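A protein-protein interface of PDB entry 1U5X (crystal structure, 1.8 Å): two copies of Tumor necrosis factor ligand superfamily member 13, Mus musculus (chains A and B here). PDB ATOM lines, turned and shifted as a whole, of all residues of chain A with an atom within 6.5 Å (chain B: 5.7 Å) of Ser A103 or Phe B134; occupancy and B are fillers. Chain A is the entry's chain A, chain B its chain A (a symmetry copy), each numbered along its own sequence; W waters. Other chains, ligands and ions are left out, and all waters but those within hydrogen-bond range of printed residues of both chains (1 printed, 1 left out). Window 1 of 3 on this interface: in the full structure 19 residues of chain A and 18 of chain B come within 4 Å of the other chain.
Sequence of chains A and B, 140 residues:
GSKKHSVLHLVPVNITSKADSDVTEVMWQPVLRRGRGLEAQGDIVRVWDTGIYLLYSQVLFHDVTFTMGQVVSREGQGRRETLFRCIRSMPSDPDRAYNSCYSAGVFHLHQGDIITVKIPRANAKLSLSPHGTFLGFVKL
Water W1 lies within hydrogen-bond range of the backbone carbonyl oxygen (O) of Pro B130 (2.7 Å), a ring nitrogen (NE2) of His B9 (2.9 Å) and the backbone carbonyl oxygen (O) of Leu A83 (3.0 Å).
Tyr B102 touches its own counterpart, Tyr A102.
4 positions are printed for both chains.
The backbone carbonyl oxygen (O) of Arg A85 lies within hydrogen-bond range of the side-chain amide nitrogen (NE2) of Gln B58, 2.9 Å away.
The backbone carbonyl oxygen (O) of His B131 sits at hydrogen-bond distance from the backbone NH (N) of Arg A85, 3.0 Å away.
The side-chain hydroxyl (OG) of Ser A103 lies within hydrogen-bond range of the side-chain amide oxygen (OE1) of Gln B58 (2.6 Å).
The backbone NH (N) of Val A106 is in hydrogen-bond range of the side-chain hydroxyl (OH) of Tyr B56, 3.1 Å away.
N of Leu A55 is in hydrogen-bond range of O of Gly A105, 2.9 Å away.
The backbone carbonyl oxygen (O) of Ser A103 lies within hydrogen-bond range of the backbone NH (N) of Ser A57 (2.9 Å).
The backbone carbonyl oxygen (O) of Val A72 is in hydrogen-bond range of the backbone NH (N) of Leu A83, at 2.8 Å.
The side-chain sulfur of Cys A86 is in hydrogen-bond range of the backbone NH of Tyr A102.
The side-chain amide nitrogen (NE2) of Gln B58 lies within hydrogen-bond range of the backbone carbonyl oxygen (O) of Gly B132 (2.9 Å).
The side-chain sulfur (SG) of Cys A86 forms a disulfide with the side-chain sulfur (SG) of Cys A101, at 2.0 Å.
Among the printed residues, merely in contact across the chains: Leu A83 with His B131, Phe A84 with His B131, Phe A84 with Phe B134, Tyr A102 with Tyr B102, Ser A103 with Phe B134, Ala A104 with Tyr B102, Ala A104 with Phe B134, Gly A105 with Tyr B56, Val A106 with His B9 and Phe A107 with His B9.
Printed residues of chain B that touch a printed residue of chain A: His B9, Tyr B56, Gln B58, Tyr B102, His B131 and Phe B134.
Hydrophobic or aromatic side chains of chain A within 4 Å of the printed part of chain B: Phe A84, Tyr A102, Ala A104, Val A106 and Phe A107.
Among the printed residues, no Asp or Glu carboxylate lies within 4 Å of a Lys or Arg side-chain nitrogen of the other chain.
Ser A103 touches just these residues of chain B: Gln B58 (2.6 Å) and Phe B134 (3.6 Å).
Printed residues of chain B within 4 Å of Phe A84: His B131 (3.4 Å) and Phe B134 (3.9 Å).
Printed residues of chain B within 4 Å of Phe A107: His B9 (3.99 Å).
Of the printed residues of chain B, Leu A83 touches His B131 (3.9 Å).
Printed residues of chain A within 4 Å of Tyr B102: Tyr A102 and Ala A104.
Tyr A56 touches none of the printed residues of chain B.
The nearest residue of chain B that does not touch Ser A103 is Tyr B102 (4.1 Å).
The nearest printed residue of chain A that does not touch Tyr B102 is Ser A103 (4.1 Å).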
ATOM      1  N   LEU A  55     -37.816  -9.539 -24.719  1.00  0.00           N
ATOM      2  CA  LEU A  55     -38.147  -8.138 -24.849  1.00  0.00           C
ATOM      3  C   LEU A  55     -37.708  -7.729 -26.234  1.00  0.00           C
ATOM      4  O   LEU A  55     -36.581  -7.956 -26.615  1.00  0.00           O
ATOM      5  CB  LEU A  55     -37.364  -7.328 -23.798  1.00  0.00           C
ATOM      6  CG  LEU A  55     -37.684  -5.900 -23.414  1.00  0.00           C
ATOM      7  CD1 LEU A  55     -39.120  -5.513 -23.555  1.00  0.00           C
ATOM      8  CD2 LEU A  55     -37.188  -5.671 -21.975  1.00  0.00           C
ATOM      9  N   TYR A  56     -38.601  -7.103 -26.983  1.00  0.00           N
ATOM     10  CA  TYR A  56     -38.269  -6.641 -28.334  1.00  0.00           C
ATOM     11  C   TYR A  56     -38.696  -5.187 -28.469  1.00  0.00           C
ATOM     12  O   TYR A  56     -39.666  -4.750 -27.848  1.00  0.00           O
ATOM     13  CB  TYR A  56     -38.909  -7.515 -29.418  1.00  0.00           C
ATOM     14  CG  TYR A  56     -40.424  -7.616 -29.405  1.00  0.00           C
ATOM     15  CD1 TYR A  56     -41.208  -6.694 -30.047  1.00  0.00           C
ATOM     16  CD2 TYR A  56     -41.039  -8.677 -28.739  1.00  0.00           C
ATOM     17  CE1 TYR A  56     -42.614  -6.814 -30.044  1.00  0.00           C
ATOM     18  CE2 TYR A  56     -42.409  -8.816 -28.692  1.00  0.00           C
ATOM     19  CZ  TYR A  56     -43.198  -7.888 -29.377  1.00  0.00           C
ATOM     20  OH  TYR A  56     -44.559  -8.047 -29.314  1.00  0.00           O
ATOM     21  N   SER A  57     -37.965  -4.446 -29.300  1.00  0.00           N
ATOM     22  CA  SER A  57     -38.156  -3.022 -29.489  1.00  0.00           C
ATOM     23  C   SER A  57     -37.836  -2.677 -30.924  1.00  0.00           C
ATOM     24  O   SER A  57     -36.782  -3.031 -31.432  1.00  0.00           O
ATOM     25  CB  SER A  57     -37.223  -2.239 -28.582  1.00  0.00           C
ATOM     26  OG  SER A  57     -37.156  -0.871 -28.963  1.00  0.00           O
ATOM     27  N   GLN A  58     -38.749  -1.976 -31.581  1.00  0.00           N
ATOM     28  CA  GLN A  58     -38.464  -1.363 -32.858  1.00  0.00           C
ATOM     29  C   GLN A  58     -38.811   0.100 -32.780  1.00  0.00           C
ATOM     30  O   GLN A  58     -39.836   0.497 -32.188  1.00  0.00           O
ATOM     31  CB  GLN A  58     -39.246  -1.973 -34.024  1.00  0.00           C
ATOM     32  CG  GLN A  58     -38.829  -1.414 -35.420  1.00  0.00           C
ATOM     33  CD  GLN A  58     -39.431  -2.214 -36.566  1.00  0.00           C
ATOM     34  OE1 GLN A  58     -38.984  -3.361 -36.814  1.00  0.00           O
ATOM     35  NE2 GLN A  58     -40.365  -1.615 -37.302  1.00  0.00           N
ATOM     36  N   GLN A  70     -32.159   3.369 -30.286  1.00  0.00           N
ATOM     37  CA  GLN A  70     -32.873   3.349 -29.025  1.00  0.00           C
ATOM     38  C   GLN A  70     -32.124   2.495 -28.032  1.00  0.00           C
ATOM     39  O   GLN A  70     -31.438   1.576 -28.405  1.00  0.00           O
ATOM     40  CB  GLN A  70     -34.298   2.864 -29.179  1.00  0.00           C
ATOM     41  CG  GLN A  70     -34.479   1.381 -29.403  1.00  0.00           C
ATOM     42  CD  GLN A  70     -34.534   1.054 -30.850  1.00  0.00           C
ATOM     43  OE1 GLN A  70     -33.941   1.780 -31.698  1.00  0.00           O
ATOM     44  NE2 GLN A  70     -35.232  -0.034 -31.170  1.00  0.00           N
ATOM     45  N   VAL A  72     -32.745   0.306 -24.441  1.00  0.00           N
ATOM     46  CA  VAL A  72     -33.711  -0.336 -23.550  1.00  0.00           C
ATOM     47  C   VAL A  72     -33.026  -0.759 -22.260  1.00  0.00           C
ATOM     48  O   VAL A  72     -32.037  -1.478 -22.306  1.00  0.00           O
ATOM     49  CB  VAL A  72     -34.326  -1.600 -24.216  1.00  0.00           C
ATOM     50  CG1 VAL A  72     -35.321  -2.290 -23.316  1.00  0.00           C
ATOM     51  CG2 VAL A  72     -35.013  -1.242 -25.559  1.00  0.00           C
ATOM     52  N   LEU A  83     -30.107  -3.037 -21.050  1.00  0.00           N
ATOM     53  CA  LEU A  83     -30.351  -4.396 -21.506  1.00  0.00           C
ATOM     54  C   LEU A  83     -29.830  -4.596 -22.926  1.00  0.00           C
ATOM     55  O   LEU A  83     -29.026  -5.488 -23.184  1.00  0.00           O
ATOM     56  CB  LEU A  83     -31.813  -4.745 -21.388  1.00  0.00           C
ATOM     57  CG  LEU A  83     -32.405  -4.674 -19.967  1.00  0.00           C
ATOM     58  CD1 LEU A  83     -33.856  -5.141 -19.996  1.00  0.00           C
ATOM     59  CD2 LEU A  83     -31.626  -5.465 -18.977  1.00  0.00           C
ATOM     60  N   PHE A  84     -30.295  -3.780 -23.848  1.00  0.00           N
ATOM     61  CA  PHE A  84     -29.757  -3.789 -25.186  1.00  0.00           C
ATOM     62  C   PHE A  84     -29.990  -2.465 -25.881  1.00  0.00           C
ATOM     63  O   PHE A  84     -30.811  -1.666 -25.453  1.00  0.00           O
ATOM     64  CB  PHE A  84     -30.403  -4.906 -26.011  1.00  0.00           C
ATOM     65  CG  PHE A  84     -31.884  -4.802 -26.167  1.00  0.00           C
ATOM     66  CD1 PHE A  84     -32.718  -5.375 -25.218  1.00  0.00           C
ATOM     67  CD2 PHE A  84     -32.468  -4.182 -27.266  1.00  0.00           C
ATOM     68  CE1 PHE A  84     -34.106  -5.341 -25.347  1.00  0.00           C
ATOM     69  CE2 PHE A  84     -33.863  -4.150 -27.418  1.00  0.00           C
ATOM     70  CZ  PHE A  84     -34.684  -4.738 -26.451  1.00  0.00           C
ATOM     71  N   ARG A  85     -29.291  -2.257 -26.986  1.00  0.00           N
ATOM     72  CA  ARG A  85     -29.503  -1.066 -27.821  1.00  0.00           C
ATOM     73  C   ARG A  85     -29.502  -1.442 -29.315  1.00  0.00           C
ATOM     74  O   ARG A  85     -28.961  -2.456 -29.712  1.00  0.00           O
ATOM     75  CB  ARG A  85     -28.494   0.023 -27.453  1.00  0.00           C
ATOM     76  CG  ARG A  85     -27.272   0.082 -28.347  1.00  0.00           C
ATOM     77  CD  ARG A  85     -26.049   0.877 -27.817  1.00  0.00           C
ATOM     78  NE  ARG A  85     -26.330   2.169 -27.184  1.00  0.00           N
ATOM     79  CZ  ARG A  85     -25.968   2.521 -25.946  1.00  0.00           C
ATOM     80  NH1 ARG A  85     -25.323   1.684 -25.138  1.00  0.00           N
ATOM     81  NH2 ARG A  85     -26.257   3.735 -25.503  1.00  0.00           N
ATOM     82  N   CYS A  86     -30.146  -0.613 -30.112  1.00  0.00           N
ATOM     83  CA  CYS A  86     -30.141  -0.719 -31.557  1.00  0.00           C
ATOM     84  C   CYS A  86     -29.477   0.545 -32.082  1.00  0.00           C
ATOM     85  O   CYS A  86     -29.691   1.607 -31.512  1.00  0.00           O
ATOM     86  CB  CYS A  86     -31.579  -0.833 -32.024  1.00  0.00           C
ATOM     87  SG  CYS A  86     -31.667  -1.247 -33.746  1.00  0.00           S
ATOM     88  N   CYS A 101     -35.124   0.388 -36.697  1.00  0.00           N
ATOM     89  CA  CYS A 101     -34.078  -0.216 -35.901  1.00  0.00           C
ATOM     90  C   CYS A 101     -34.760  -1.198 -34.979  1.00  0.00           C
ATOM     91  O   CYS A 101     -35.500  -0.809 -34.098  1.00  0.00           O
ATOM     92  CB  CYS A 101     -33.335   0.874 -35.127  1.00  0.00           C
ATOM     93  SG  CYS A 101     -31.636   0.478 -34.787  1.00  0.00           S
ATOM     94  N   TYR A 102     -34.519  -2.487 -35.198  1.00  0.00           N
ATOM     95  CA  TYR A 102     -35.108  -3.539 -34.352  1.00  0.00           C
ATOM     96  C   TYR A 102     -34.013  -4.227 -33.534  1.00  0.00           C
ATOM     97  O   TYR A 102     -32.943  -4.544 -34.065  1.00  0.00           O
ATOM     98  CB  TYR A 102     -35.788  -4.592 -35.246  1.00  0.00           C
ATOM     99  CG  TYR A 102     -36.446  -5.742 -34.497  1.00  0.00           C
ATOM    100  CD1 TYR A 102     -35.691  -6.832 -34.048  1.00  0.00           C
ATOM    101  CD2 TYR A 102     -37.810  -5.726 -34.185  1.00  0.00           C
ATOM    102  CE1 TYR A 102     -36.281  -7.884 -33.320  1.00  0.00           C
ATOM    103  CE2 TYR A 102     -38.385  -6.794 -33.467  1.00  0.00           C
ATOM    104  CZ  TYR A 102     -37.645  -7.851 -33.063  1.00  0.00           C
ATOM    105  OH  TYR A 102     -38.131  -8.941 -32.349  1.00  0.00           O
ATOM    106  N   SER A 103     -34.294  -4.484 -32.259  1.00  0.00           N
ATOM    107  CA  SER A 103     -33.437  -5.371 -31.439  1.00  0.00           C
ATOM    108  C   SER A 103     -34.281  -6.060 -30.406  1.00  0.00           C
ATOM    109  O   SER A 103     -35.427  -5.661 -30.142  1.00  0.00           O
ATOM    110  CB  SER A 103     -32.274  -4.577 -30.814  1.00  0.00           C
ATOM    111  OG  SER A 103     -31.364  -5.422 -30.110  1.00  0.00           O
ATOM    112  N   ALA A 104     -33.757  -7.137 -29.866  1.00  0.00           N
ATOM    113  CA  ALA A 104     -34.508  -7.945 -28.907  1.00  0.00           C
ATOM    114  C   ALA A 104     -33.556  -8.896 -28.197  1.00  0.00           C
ATOM    115  O   ALA A 104     -32.490  -9.244 -28.708  1.00  0.00           O
ATOM    116  CB  ALA A 104     -35.558  -8.761 -29.626  1.00  0.00           C
ATOM    117  N   GLY A 105     -33.934  -9.313 -27.013  1.00  0.00           N
ATOM    118  CA  GLY A 105     -33.195 -10.326 -26.289  1.00  0.00           C
ATOM    119  C   GLY A 105     -33.927 -10.857 -25.095  1.00  0.00           C
ATOM    120  O   GLY A 105     -35.029 -10.390 -24.800  1.00  0.00           O
ATOM    121  N   VAL A 106     -33.307 -11.821 -24.415  1.00  0.00           N
ATOM    122  CA  VAL A 106     -33.941 -12.489 -23.297  1.00  0.00           C
ATOM    123  C   VAL A 106     -33.264 -12.088 -22.008  1.00  0.00           C
ATOM    124  O   VAL A 106     -32.052 -12.196 -21.903  1.00  0.00           O
ATOM    125  CB  VAL A 106     -33.906 -14.000 -23.436  1.00  0.00           C
ATOM    126  CG1 VAL A 106     -34.550 -14.647 -22.258  1.00  0.00           C
ATOM    127  CG2 VAL A 106     -34.662 -14.397 -24.664  1.00  0.00           C
ATOM    128  N   PHE A 107     -34.074 -11.628 -21.045  1.00  0.00           N
ATOM    129  CA  PHE A 107     -33.555 -11.056 -19.811  1.00  0.00           C
ATOM    130  C   PHE A 107     -34.371 -11.449 -18.596  1.00  0.00           C
ATOM    131  O   PHE A 107     -35.590 -11.623 -18.671  1.00  0.00           O
ATOM    132  CB  PHE A 107     -33.553  -9.533 -19.928  1.00  0.00           C
ATOM    133  CG  PHE A 107     -32.769  -9.036 -21.089  1.00  0.00           C
ATOM    134  CD1 PHE A 107     -31.405  -8.888 -20.985  1.00  0.00           C
ATOM    135  CD2 PHE A 107     -33.399  -8.742 -22.310  1.00  0.00           C
ATOM    136  CE1 PHE A 107     -30.664  -8.466 -22.071  1.00  0.00           C
ATOM    137  CE2 PHE A 107     -32.655  -8.296 -23.394  1.00  0.00           C
ATOM    138  CZ  PHE A 107     -31.290  -8.159 -23.255  1.00  0.00           C
ATOM    139  N   HIS B   9     -28.327 -16.643 -22.845  1.00  0.00           N
ATOM    140  CA  HIS B   9     -28.007 -15.346 -23.408  1.00  0.00           C
ATOM    141  C   HIS B   9     -26.524 -15.121 -23.122  1.00  0.00           C
ATOM    142  O   HIS B   9     -26.081 -15.198 -21.982  1.00  0.00           O
ATOM    143  CB  HIS B   9     -28.858 -14.229 -22.809  1.00  0.00           C
ATOM    144  CG  HIS B   9     -28.664 -12.897 -23.459  1.00  0.00           C
ATOM    145  ND1 HIS B   9     -29.325 -12.525 -24.621  1.00  0.00           N
ATOM    146  CD2 HIS B   9     -27.893 -11.838 -23.105  1.00  0.00           C
ATOM    147  CE1 HIS B   9     -28.990 -11.277 -24.919  1.00  0.00           C
ATOM    148  NE2 HIS B   9     -28.119 -10.842 -24.021  1.00  0.00           N
ATOM    149  N   LEU B  10     -25.789 -14.850 -24.192  1.00  0.00           N
ATOM    150  CA  LEU B  10     -24.342 -14.748 -24.211  1.00  0.00           C
ATOM    151  C   LEU B  10     -23.896 -13.385 -24.713  1.00  0.00           C
ATOM    152  O   LEU B  10     -24.552 -12.781 -25.600  1.00  0.00           O
ATOM    153  CB  LEU B  10     -23.796 -15.779 -25.189  1.00  0.00           C
ATOM    154  CG  LEU B  10     -24.198 -17.229 -24.987  1.00  0.00           C
ATOM    155  CD1 LEU B  10     -24.027 -17.993 -26.295  1.00  0.00           C
ATOM    156  CD2 LEU B  10     -23.364 -17.848 -23.902  1.00  0.00           C
ATOM    157  N   VAL B  11     -22.796 -12.910 -24.148  1.00  0.00           N
ATOM    158  CA  VAL B  11     -22.204 -11.639 -24.540  1.00  0.00           C
ATOM    159  C   VAL B  11     -20.703 -11.811 -24.754  1.00  0.00           C
ATOM    160  O   VAL B  11     -20.136 -12.845 -24.388  1.00  0.00           O
ATOM    161  CB  VAL B  11     -22.490 -10.554 -23.481  1.00  0.00           C
ATOM    162  CG1 VAL B  11     -24.003 -10.373 -23.323  1.00  0.00           C
ATOM    163  CG2 VAL B  11     -21.833 -10.880 -22.170  1.00  0.00           C
ATOM    164  N   PRO B  12     -20.032 -10.839 -25.371  1.00  0.00           N
ATOM    165  CA  PRO B  12     -18.606 -11.011 -25.647  1.00  0.00           C
ATOM    166  C   PRO B  12     -17.686 -10.978 -24.420  1.00  0.00           C
ATOM    167  O   PRO B  12     -17.914 -10.257 -23.439  1.00  0.00           O
ATOM    168  CB  PRO B  12     -18.272  -9.834 -26.564  1.00  0.00           C
ATOM    169  CG  PRO B  12     -19.615  -9.365 -27.125  1.00  0.00           C
ATOM    170  CD  PRO B  12     -20.535  -9.581 -25.941  1.00  0.00           C
ATOM    171  N   TRP B  28     -17.487 -16.063 -26.309  1.00  0.00           N
ATOM    172  CA  TRP B  28     -18.768 -15.805 -25.620  1.00  0.00           C
ATOM    173  C   TRP B  28     -18.722 -16.226 -24.140  1.00  0.00           C
ATOM    174  O   TRP B  28     -18.001 -17.171 -23.771  1.00  0.00           O
ATOM    175  CB  TRP B  28     -19.907 -16.557 -26.306  1.00  0.00           C
ATOM    176  CG  TRP B  28     -20.156 -16.160 -27.737  1.00  0.00           C
ATOM    177  CD1 TRP B  28     -19.779 -16.851 -28.850  1.00  0.00           C
ATOM    178  CD2 TRP B  28     -20.787 -14.962 -28.204  1.00  0.00           C
ATOM    179  NE1 TRP B  28     -20.155 -16.169 -29.981  1.00  0.00           N
ATOM    180  CE2 TRP B  28     -20.757 -14.997 -29.618  1.00  0.00           C
ATOM    181  CE3 TRP B  28     -21.350 -13.842 -27.572  1.00  0.00           C
ATOM    182  CZ2 TRP B  28     -21.281 -13.977 -30.407  1.00  0.00           C
ATOM    183  CZ3 TRP B  28     -21.880 -12.824 -28.368  1.00  0.00           C
ATOM    184  CH2 TRP B  28     -21.842 -12.905 -29.768  1.00  0.00           C
ATOM    185  N   TYR B  56     -31.069 -16.060 -31.805  1.00  0.00           N
ATOM    186  CA  TYR B  56     -30.969 -14.649 -32.187  1.00  0.00           C
ATOM    187  C   TYR B  56     -29.523 -14.204 -32.037  1.00  0.00           C
ATOM    188  O   TYR B  56     -28.791 -14.703 -31.179  1.00  0.00           O
ATOM    189  CB  TYR B  56     -31.915 -13.760 -31.371  1.00  0.00           C
ATOM    190  CG  TYR B  56     -31.726 -13.768 -29.865  1.00  0.00           C
ATOM    191  CD1 TYR B  56     -30.828 -12.933 -29.253  1.00  0.00           C
ATOM    192  CD2 TYR B  56     -32.489 -14.630 -29.077  1.00  0.00           C
ATOM    193  CE1 TYR B  56     -30.680 -12.936 -27.850  1.00  0.00           C
ATOM    194  CE2 TYR B  56     -32.357 -14.681 -27.707  1.00  0.00           C
ATOM    195  CZ  TYR B  56     -31.462 -13.803 -27.090  1.00  0.00           C
ATOM    196  OH  TYR B  56     -31.346 -13.874 -25.725  1.00  0.00           O
ATOM    197  N   SER B  57     -29.122 -13.250 -32.875  1.00  0.00           N
ATOM    198  CA  SER B  57     -27.759 -12.763 -32.949  1.00  0.00           C
ATOM    199  C   SER B  57     -27.788 -11.294 -33.295  1.00  0.00           C
ATOM    200  O   SER B  57     -28.432 -10.890 -34.253  1.00  0.00           O
ATOM    201  CB  SER B  57     -26.993 -13.502 -34.032  1.00  0.00           C
ATOM    202  OG  SER B  57     -25.772 -12.844 -34.344  1.00  0.00           O
ATOM    203  N   GLN B  58     -27.082 -10.488 -32.515  1.00  0.00           N
ATOM    204  CA  GLN B  58     -26.814  -9.116 -32.881  1.00  0.00           C
ATOM    205  C   GLN B  58     -25.329  -8.879 -32.816  1.00  0.00           C
ATOM    206  O   GLN B  58     -24.632  -9.357 -31.896  1.00  0.00           O
ATOM    207  CB  GLN B  58     -27.496  -8.090 -31.973  1.00  0.00           C
ATOM    208  CG  GLN B  58     -27.330  -6.615 -32.456  1.00  0.00           C
ATOM    209  CD  GLN B  58     -28.224  -5.652 -31.690  1.00  0.00           C
ATOM    210  OE1 GLN B  58     -29.461  -5.658 -31.909  1.00  0.00           O
ATOM    211  NE2 GLN B  58     -27.629  -4.791 -30.868  1.00  0.00           N
ATOM    212  N   VAL B  59     -24.847  -8.149 -33.805  1.00  0.00           N
ATOM    213  CA  VAL B  59     -23.476  -7.649 -33.770  1.00  0.00           C
ATOM    214  C   VAL B  59     -23.493  -6.157 -34.035  1.00  0.00           C
ATOM    215  O   VAL B  59     -24.169  -5.667 -34.958  1.00  0.00           O
ATOM    216  CB  VAL B  59     -22.555  -8.396 -34.776  1.00  0.00           C
ATOM    217  CG1 VAL B  59     -21.129  -7.817 -34.711  1.00  0.00           C
ATOM    218  CG2 VAL B  59     -22.560  -9.907 -34.540  1.00  0.00           C
ATOM    219  N   TYR B 102     -29.121  -7.134 -36.494  1.00  0.00           N
ATOM    220  CA  TYR B 102     -29.843  -8.171 -35.738  1.00  0.00           C
ATOM    221  C   TYR B 102     -30.537  -9.134 -36.703  1.00  0.00           C
ATOM    222  O   TYR B 102     -31.153  -8.700 -37.683  1.00  0.00           O
ATOM    223  CB  TYR B 102     -30.913  -7.506 -34.853  1.00  0.00           C
ATOM    224  CG  TYR B 102     -31.737  -8.467 -34.008  1.00  0.00           C
ATOM    225  CD1 TYR B 102     -32.831  -9.148 -34.556  1.00  0.00           C
ATOM    226  CD2 TYR B 102     -31.402  -8.744 -32.679  1.00  0.00           C
ATOM    227  CE1 TYR B 102     -33.578 -10.070 -33.797  1.00  0.00           C
ATOM    228  CE2 TYR B 102     -32.169  -9.661 -31.931  1.00  0.00           C
ATOM    229  CZ  TYR B 102     -33.237 -10.289 -32.469  1.00  0.00           C
ATOM    230  OH  TYR B 102     -34.043 -11.208 -31.804  1.00  0.00           O
ATOM    231  N   SER B 129     -19.359  -4.583 -26.369  1.00  0.00           N
ATOM    232  CA  SER B 129     -20.390  -4.189 -25.430  1.00  0.00           C
ATOM    233  C   SER B 129     -21.457  -5.248 -25.399  1.00  0.00           C
ATOM    234  O   SER B 129     -21.953  -5.630 -26.468  1.00  0.00           O
ATOM    235  CB  SER B 129     -21.034  -2.864 -25.818  1.00  0.00           C
ATOM    236  OG  SER B 129     -22.218  -2.668 -25.078  1.00  0.00           O
ATOM    237  N   PRO B 130     -21.851  -5.700 -24.201  1.00  0.00           N
ATOM    238  CA  PRO B 130     -22.905  -6.723 -24.072  1.00  0.00           C
ATOM    239  C   PRO B 130     -24.272  -6.214 -24.526  1.00  0.00           C
ATOM    240  O   PRO B 130     -25.160  -6.998 -24.906  1.00  0.00           O
ATOM    241  CB  PRO B 130     -22.879  -7.062 -22.565  1.00  0.00           C
ATOM    242  CG  PRO B 130     -22.350  -5.836 -21.912  1.00  0.00           C
ATOM    243  CD  PRO B 130     -21.366  -5.243 -22.886  1.00  0.00           C
ATOM    244  N   HIS B 131     -24.436  -4.892 -24.554  1.00  0.00           N
ATOM    245  CA  HIS B 131     -25.711  -4.269 -24.997  1.00  0.00           C
ATOM    246  C   HIS B 131     -25.804  -4.186 -26.502  1.00  0.00           C
ATOM    247  O   HIS B 131     -26.906  -4.087 -27.021  1.00  0.00           O
ATOM    248  CB  HIS B 131     -25.864  -2.866 -24.355  1.00  0.00           C
ATOM    249  CG  HIS B 131     -25.469  -2.860 -22.929  1.00  0.00           C
ATOM    250  ND1 HIS B 131     -24.278  -2.322 -22.487  1.00  0.00           N
ATOM    251  CD2 HIS B 131     -26.061  -3.403 -21.846  1.00  0.00           C
ATOM    252  CE1 HIS B 131     -24.179  -2.495 -21.182  1.00  0.00           C
ATOM    253  NE2 HIS B 131     -25.246  -3.151 -20.769  1.00  0.00           N
ATOM    254  N   GLY B 132     -24.659  -4.282 -27.202  1.00  0.00           N
ATOM    255  CA  GLY B 132     -24.615  -4.191 -28.654  1.00  0.00           C
ATOM    256  C   GLY B 132     -24.334  -5.454 -29.467  1.00  0.00           C
ATOM    257  O   GLY B 132     -24.805  -5.586 -30.600  1.00  0.00           O
ATOM    258  N   THR B 133     -23.585  -6.378 -28.885  1.00  0.00           N
ATOM    259  CA  THR B 133     -23.226  -7.641 -29.526  1.00  0.00           C
ATOM    260  C   THR B 133     -23.631  -8.746 -28.557  1.00  0.00           C
ATOM    261  O   THR B 133     -23.196  -8.757 -27.424  1.00  0.00           O
ATOM    262  CB  THR B 133     -21.728  -7.670 -29.794  1.00  0.00           C
ATOM    263  OG1 THR B 133     -21.410  -6.621 -30.695  1.00  0.00           O
ATOM    264  CG2 THR B 133     -21.299  -8.915 -30.499  1.00  0.00           C
ATOM    265  N   PHE B 134     -24.501  -9.640 -29.005  1.00  0.00           N
ATOM    266  CA  PHE B 134     -24.988 -10.716 -28.179  1.00  0.00           C
ATOM    267  C   PHE B 134     -25.538 -11.859 -29.010  1.00  0.00           C
ATOM    268  O   PHE B 134     -25.733 -11.739 -30.219  1.00  0.00           O
ATOM    269  CB  PHE B 134     -25.990 -10.175 -27.139  1.00  0.00           C
ATOM    270  CG  PHE B 134     -27.133  -9.395 -27.718  1.00  0.00           C
ATOM    271  CD1 PHE B 134     -28.219 -10.042 -28.272  1.00  0.00           C
ATOM    272  CD2 PHE B 134     -27.148  -8.005 -27.642  1.00  0.00           C
ATOM    273  CE1 PHE B 134     -29.289  -9.319 -28.791  1.00  0.00           C
ATOM    274  CE2 PHE B 134     -28.216  -7.304 -28.161  1.00  0.00           C
ATOM    275  CZ  PHE B 134     -29.271  -7.942 -28.693  1.00  0.00           C
ATOM    276  N   LEU B 135     -25.740 -12.981 -28.341  1.00  0.00           N
ATOM    277  CA  LEU B 135     -26.156 -14.214 -28.979  1.00  0.00           C
ATOM    278  C   LEU B 135     -27.034 -14.962 -28.002  1.00  0.00           C
ATOM    279  O   LEU B 135     -26.687 -15.122 -26.831  1.00  0.00           O
ATOM    280  CB  LEU B 135     -24.934 -15.082 -29.308  1.00  0.00           C
ATOM    281  CG  LEU B 135     -25.246 -16.469 -29.929  1.00  0.00           C
ATOM    282  CD1 LEU B 135     -25.884 -16.340 -31.296  1.00  0.00           C
ATOM    283  CD2 LEU B 135     -23.937 -17.291 -30.013  1.00  0.00           C
ATOM    284  N   GLY B 136     -28.188 -15.424 -28.459  1.00  0.00           N
ATOM    285  CA  GLY B 136     -29.016 -16.184 -27.555  1.00  0.00           C
ATOM    286  C   GLY B 136     -29.916 -17.238 -28.151  1.00  0.00           C
ATOM    287  O   GLY B 136     -30.114 -17.317 -29.356  1.00  0.00           O
HETATM  288  O   HOH W   1     -27.439  -7.996 -23.834  1.00  0.00           O
